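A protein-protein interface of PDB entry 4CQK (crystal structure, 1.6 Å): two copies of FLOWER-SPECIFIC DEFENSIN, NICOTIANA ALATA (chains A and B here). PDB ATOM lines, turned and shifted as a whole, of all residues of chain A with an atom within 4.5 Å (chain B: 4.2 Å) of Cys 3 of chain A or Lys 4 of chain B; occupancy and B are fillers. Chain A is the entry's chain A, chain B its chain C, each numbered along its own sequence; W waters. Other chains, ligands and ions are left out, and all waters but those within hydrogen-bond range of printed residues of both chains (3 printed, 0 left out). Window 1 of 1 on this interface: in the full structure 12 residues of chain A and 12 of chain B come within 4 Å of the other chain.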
ATOM      1  N   GLU A   2      20.018   3.465 -25.458  1.00  0.00           N
ATOM      2  CA  GLU A   2      20.451   3.809 -24.105  1.00  0.00           C
ATOM      3  C   GLU A   2      19.726   5.073 -23.724  1.00  0.00           C
ATOM      4  O   GLU A   2      19.207   5.817 -24.591  1.00  0.00           O
ATOM      5  CB  GLU A   2      21.954   4.070 -24.018  1.00  0.00           C
ATOM      6  CG  GLU A   2      22.800   2.901 -24.441  1.00  0.00           C
ATOM      7  CD  GLU A   2      24.231   3.087 -24.029  1.00  0.00           C
ATOM      8  OE1 GLU A   2      24.976   3.726 -24.790  1.00  0.00           O
ATOM      9  OE2 GLU A   2      24.594   2.618 -22.930  1.00  0.00           O
ATOM     10  N   CYS A   3      19.690   5.334 -22.431  1.00  0.00           N
ATOM     11  CA  CYS A   3      19.101   6.562 -21.936  1.00  0.00           C
ATOM     12  C   CYS A   3      20.241   7.569 -21.881  1.00  0.00           C
ATOM     13  O   CYS A   3      21.354   7.236 -21.465  1.00  0.00           O
ATOM     14  CB  CYS A   3      18.407   6.336 -20.594  1.00  0.00           C
ATOM     15  SG  CYS A   3      16.722   5.674 -20.874  1.00  0.00           S
ATOM     16  N   LYS A   4      19.985   8.784 -22.357  1.00  0.00           N
ATOM     17  CA  LYS A   4      21.067   9.748 -22.548  1.00  0.00           C
ATOM     18  C   LYS A   4      20.654  11.128 -22.032  1.00  0.00           C
ATOM     19  O   LYS A   4      19.497  11.515 -22.133  1.00  0.00           O
ATOM     20  CB  LYS A   4      21.400   9.812 -24.043  1.00  0.00           C
ATOM     21  CG  LYS A   4      22.496  10.754 -24.401  1.00  0.00           C
ATOM     22  CD  LYS A   4      23.055  10.409 -25.784  1.00  0.00           C
ATOM     23  CE  LYS A   4      22.019  10.553 -26.892  1.00  0.00           C
ATOM     24  NZ  LYS A   4      22.414   9.686 -28.045  1.00  0.00           N
ATOM     25  N   CYS A  43      25.974  11.904 -21.274  1.00  0.00           N
ATOM     26  CA  CYS A  43      26.134  10.691 -20.463  1.00  0.00           C
ATOM     27  C   CYS A  43      25.086   9.659 -20.857  1.00  0.00           C
ATOM     28  O   CYS A  43      23.976  10.031 -21.248  1.00  0.00           O
ATOM     29  CB  CYS A  43      25.897  11.033 -18.983  1.00  0.00           C
ATOM     30  SG  CYS A  43      27.058  12.296 -18.336  1.00  0.00           S
ATOM     31  N   THR A  44      25.411   8.370 -20.720  1.00  0.00           N
ATOM     32  CA  THR A  44      24.471   7.333 -21.131  1.00  0.00           C
ATOM     33  C   THR A  44      24.447   6.229 -20.099  1.00  0.00           C
ATOM     34  O   THR A  44      25.443   5.996 -19.418  1.00  0.00           O
ATOM     35  CB  THR A  44      24.848   6.725 -22.498  1.00  0.00           C
ATOM     36  OG1 THR A  44      26.225   6.327 -22.483  1.00  0.00           O
ATOM     37  CG2 THR A  44      24.648   7.741 -23.618  1.00  0.00           C
ATOM     38  N   LYS A  45      23.312   5.531 -20.020  1.00  0.00           N
ATOM     39  CA  LYS A  45      23.176   4.361 -19.149  1.00  0.00           C
ATOM     40  C   LYS A  45      22.009   3.548 -19.672  1.00  0.00           C
ATOM     41  O   LYS A  45      21.242   4.034 -20.497  1.00  0.00           O
ATOM     42  CB  LYS A  45      22.928   4.801 -17.697  1.00  0.00           C
ATOM     43  CG  LYS A  45      21.623   5.568 -17.486  1.00  0.00           C
ATOM     44  CD  LYS A  45      21.449   5.917 -16.010  1.00  0.00           C
ATOM     45  CE  LYS A  45      20.125   6.661 -15.767  1.00  0.00           C
ATOM     46  NZ  LYS A  45      19.932   6.996 -14.309  1.00  0.00           N
ATOM     47  N   PRO A  46      21.858   2.303 -19.203  1.00  0.00           N
ATOM     48  CA  PRO A  46      20.708   1.508 -19.675  1.00  0.00           C
ATOM     49  C   PRO A  46      19.393   2.146 -19.252  1.00  0.00           C
ATOM     50  O   PRO A  46      19.329   2.771 -18.190  1.00  0.00           O
ATOM     51  CB  PRO A  46      20.875   0.169 -18.949  1.00  0.00           C
ATOM     52  CG  PRO A  46      22.315   0.106 -18.591  1.00  0.00           C
ATOM     53  CD  PRO A  46      22.761   1.537 -18.335  1.00  0.00           C
ATOM     54  N   CYS A  47      18.354   2.023 -20.072  1.00  0.00           N
ATOM     55  CA  CYS A  47      17.052   2.537 -19.667  1.00  0.00           C
ATOM     56  C   CYS A  47      16.433   1.684 -18.565  1.00  0.00           C
ATOM     57  O   CYS A  47      15.527   2.155 -17.868  1.00  0.00           O
ATOM     58  CB  CYS A  47      16.118   2.610 -20.865  1.00  0.00           C
ATOM     59  SG  CYS A  47      16.646   3.901 -22.006  1.00  0.00           S
ATOM     60  OXT CYS A  47      16.818   0.525 -18.342  1.00  0.00           O
ATOM     61  N   GLU B   2      16.617  15.704 -18.497  1.00  0.00           N
ATOM     62  CA  GLU B   2      15.881  14.439 -18.462  1.00  0.00           C
ATOM     63  C   GLU B   2      16.703  13.378 -19.149  1.00  0.00           C
ATOM     64  O   GLU B   2      17.605  13.688 -19.937  1.00  0.00           O
ATOM     65  CB  GLU B   2      14.534  14.553 -19.190  1.00  0.00           C
ATOM     66  CG  GLU B   2      13.607  15.626 -18.646  1.00  0.00           C
ATOM     67  CD  GLU B   2      12.291  15.682 -19.423  1.00  0.00           C
ATOM     68  OE1 GLU B   2      12.266  16.246 -20.538  1.00  0.00           O
ATOM     69  OE2 GLU B   2      11.312  15.133 -18.918  1.00  0.00           O
ATOM     70  N   CYS B   3      16.404  12.117 -18.852  1.00  0.00           N
ATOM     71  CA  CYS B   3      17.066  11.024 -19.539  1.00  0.00           C
ATOM     72  C   CYS B   3      16.125  10.664 -20.672  1.00  0.00           C
ATOM     73  O   CYS B   3      14.908  10.572 -20.458  1.00  0.00           O
ATOM     74  CB  CYS B   3      17.328   9.858 -18.601  1.00  0.00           C
ATOM     75  SG  CYS B   3      18.876  10.156 -17.619  1.00  0.00           S
ATOM     76  N   LYS B   4      16.674  10.518 -21.873  1.00  0.00           N
ATOM     77  CA  LYS B   4      15.850  10.434 -23.079  1.00  0.00           C
ATOM     78  C   LYS B   4      16.334   9.297 -23.967  1.00  0.00           C
ATOM     79  O   LYS B   4      17.549   9.021 -24.050  1.00  0.00           O
ATOM     80  CB  LYS B   4      15.937  11.752 -23.849  1.00  0.00           C
ATOM     81  CG  LYS B   4      15.041  11.840 -25.059  1.00  0.00           C
ATOM     82  CD  LYS B   4      14.865  13.315 -25.469  1.00  0.00           C
ATOM     83  CE  LYS B   4      16.188  13.941 -25.923  1.00  0.00           C
ATOM     84  NZ  LYS B   4      16.175  15.410 -25.652  1.00  0.00           N
ATOM     85  N   THR B   5      15.387   8.660 -24.656  1.00  0.00           N
ATOM     86  CA  THR B   5      15.733   7.605 -25.591  1.00  0.00           C
ATOM     87  C   THR B   5      14.612   7.507 -26.612  1.00  0.00           C
ATOM     88  O   THR B   5      13.570   8.107 -26.410  1.00  0.00           O
ATOM     89  CB  THR B   5      15.924   6.254 -24.850  1.00  0.00           C
ATOM     90  OG1 THR B   5      16.620   5.323 -25.694  1.00  0.00           O
ATOM     91  CG2 THR B   5      14.587   5.651 -24.408  1.00  0.00           C
ATOM     92  N   PHE B  29       8.379   5.116 -19.023  1.00  0.00           N
ATOM     93  CA  PHE B  29       8.909   6.482 -18.961  1.00  0.00           C
ATOM     94  C   PHE B  29       7.819   7.401 -18.427  1.00  0.00           C
ATOM     95  O   PHE B  29       6.694   6.956 -18.212  1.00  0.00           O
ATOM     96  CB  PHE B  29       9.400   6.923 -20.349  1.00  0.00           C
ATOM     97  CG  PHE B  29      10.611   6.169 -20.800  1.00  0.00           C
ATOM     98  CD1 PHE B  29      10.474   4.916 -21.378  1.00  0.00           C
ATOM     99  CD2 PHE B  29      11.884   6.701 -20.629  1.00  0.00           C
ATOM    100  CE1 PHE B  29      11.591   4.197 -21.772  1.00  0.00           C
ATOM    101  CE2 PHE B  29      13.022   5.993 -21.028  1.00  0.00           C
ATOM    102  CZ  PHE B  29      12.879   4.744 -21.597  1.00  0.00           C
ATOM    103  N   LEU B  42      10.325  10.217 -28.930  1.00  0.00           N
ATOM    104  CA  LEU B  42      11.367  10.211 -27.898  1.00  0.00           C
ATOM    105  C   LEU B  42      10.711  10.085 -26.527  1.00  0.00           C
ATOM    106  O   LEU B  42       9.798  10.851 -26.200  1.00  0.00           O
ATOM    107  CB  LEU B  42      12.176  11.508 -27.961  1.00  0.00           C
ATOM    108  CG  LEU B  42      12.836  11.758 -29.327  1.00  0.00           C
ATOM    109  CD1 LEU B  42      13.638  13.044 -29.316  1.00  0.00           C
ATOM    110  CD2 LEU B  42      13.730  10.579 -29.695  1.00  0.00           C
ATOM    111  N   CYS B  43      11.187   9.139 -25.724  1.00  0.00           N
ATOM    112  CA  CYS B  43      10.683   8.965 -24.365  1.00  0.00           C
ATOM    113  C   CYS B  43      11.612   9.635 -23.357  1.00  0.00           C
ATOM    114  O   CYS B  43      12.826   9.618 -23.539  1.00  0.00           O
ATOM    115  CB  CYS B  43      10.623   7.481 -24.023  1.00  0.00           C
ATOM    116  SG  CYS B  43       9.489   6.568 -25.123  1.00  0.00           S
ATOM    117  N   THR B  44      11.042  10.208 -22.300  1.00  0.00           N
ATOM    118  CA  THR B  44      11.828  10.882 -21.273  1.00  0.00           C
ATOM    119  C   THR B  44      11.399  10.472 -19.867  1.00  0.00           C
ATOM    120  O   THR B  44      10.234  10.110 -19.611  1.00  0.00           O
ATOM    121  CB  THR B  44      11.718  12.419 -21.392  1.00  0.00           C
ATOM    122  OG1 THR B  44      10.343  12.811 -21.287  1.00  0.00           O
ATOM    123  CG2 THR B  44      12.307  12.911 -22.725  1.00  0.00           C
ATOM    124  N   LYS B  45      12.360  10.494 -18.952  1.00  0.00           N
ATOM    125  CA  LYS B  45      12.069  10.275 -17.539  1.00  0.00           C
ATOM    126  C   LYS B  45      13.184  10.947 -16.735  1.00  0.00           C
ATOM    127  O   LYS B  45      14.217  11.321 -17.282  1.00  0.00           O
ATOM    128  CB  LYS B  45      11.983   8.773 -17.222  1.00  0.00           C
ATOM    129  CG  LYS B  45      13.324   8.037 -17.380  1.00  0.00           C
ATOM    130  CD  LYS B  45      13.185   6.527 -17.166  1.00  0.00           C
ATOM    131  CE  LYS B  45      14.521   5.829 -17.368  1.00  0.00           C
ATOM    132  NZ  LYS B  45      14.488   4.397 -16.933  1.00  0.00           N
HETATM  133  O   HOH W   1      18.202  14.214 -22.618  1.00  0.00           O
HETATM  134  O   HOH W   2      19.258   8.233 -26.362  1.00  0.00           O
HETATM  135  O   HOH W   3      17.539   4.349 -16.712  1.00  0.00           O
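O of Cys 47 of chain A is in salt-bridge range of NZ of Lys 45 of chain B, at 2.6 Å. The backbone NH (N) of Lys 4 of chain A sits at hydrogen-bond distance from the backbone carbonyl oxygen (O) of Lys 4 of chain B (3.0 Å). O of Glu 2 of chain A lies within hydrogen-bond range of OG1 of Thr 5 of chain B, at 2.9 Å.
Water W1 lies within hydrogen-bond range of the backbone carbonyl oxygen of Glu 2 of chain B (2.8 Å) and the backbone carbonyl oxygen of Lys 4 of chain A (3.0 Å). Water W3 lies within hydrogen-bond range of O of Pro 46 of chain A (2.8 Å), NZ of Lys 45 of chain B (3.1 Å) and O of Cys 47 of chain A (3.2 Å). Water W2 lies within hydrogen-bond range of O of Lys 4 of chain B (3.0 Å) and O of Glu 2 of chain A (3.0 Å).
Among the printed residues, merely in contact across the chains: Lys 4 of chain A with Cys 3 of chain B, Cys 3 of chain A with Lys 4 of chain B, Cys 47 of chain A with Thr 5 of chain B, Lys 4 of chain A with Glu 2 of chain B, Glu 2 of chain A with Lys 4 of chain B, Cys 3 of chain A with Phe 29 of chain B and Cys 47 of chain A with Phe 29 of chain B.
Cys 3 of chain A touches just these residues of chain B: Lys 4 (3.6 Å) and Phe 29 (3.7 Å). Of the printed residues of chain A, Cys 3 of chain B touches Lys 4 (3.6 Å). Printed residues of chain A within 4 Å of Glu 2 of chain B: Lys 4 (3.6 Å). Printed residues of chain A within 4 Å of Phe 29 of chain B: Cys 3 (3.7 Å) and Cys 47 (3.9 Å). Printed residues of chain B within 4 Å of Cys 47 of chain A: Thr 5, Phe 29 and Lys 45. Of the printed residues of chain A, Thr 5 of chain B touches Glu 2 and Cys 47. The nearest residue of chain B that does not touch Cys 3 of chain A is Thr 5 of chain B (4.1 Å). The nearest printed residue of chain A that does not touch Lys 4 of chain B is Cys 47 of chain A (5.6 Å).
The backbone NH of Cys 43 of chain B sits at hydrogen-bond distance from the backbone carbonyl oxygen of Thr 5 of chain B, at 2.7 Å. The backbone NH (N) of Cys 3 of chain A sits at hydrogen-bond distance from the backbone carbonyl oxygen (O) of Lys 45 of chain A, 2.8 Å away. The side-chain carboxylate (OE2) of Glu 2 of chain B is in hydrogen-bond range of the side-chain hydroxyl (OG1) of Thr 44 of chain B. The side-chain sulfur (SG) of Cys 47 of chain A is disulfide-bonded to the side-chain sulfur (SG) of Cys 3 of chain A (2.1 Å). O of Lys 45 of chain B sits at hydrogen-bond distance from N of Cys 3 of chain B (2.8 Å).
Glu 2 of chain A touches Lys 4 of chain B, and with the chains exchanged Lys 4 of chain A touches Glu 2 of chain B. Cys 3 of chain A touches Lys 4 of chain B, and with the chains exchanged Lys 4 of chain A touches Cys 3 of chain B. Lys 4 of chain B touches its own counterpart, Lys 4 of chain A. Of the 10 pairs that touch across the chains among the printed residues, 5 have their exchanged pair printed and touching as well.
Of the 8 printed residues of chain A, 4 touch a printed residue of chain B. Printed residues of chain A that touch a printed residue of chain B: Glu 2, Cys 3, Lys 4 and Cys 47. Among the printed residues, 10 pairs touch across the chains.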
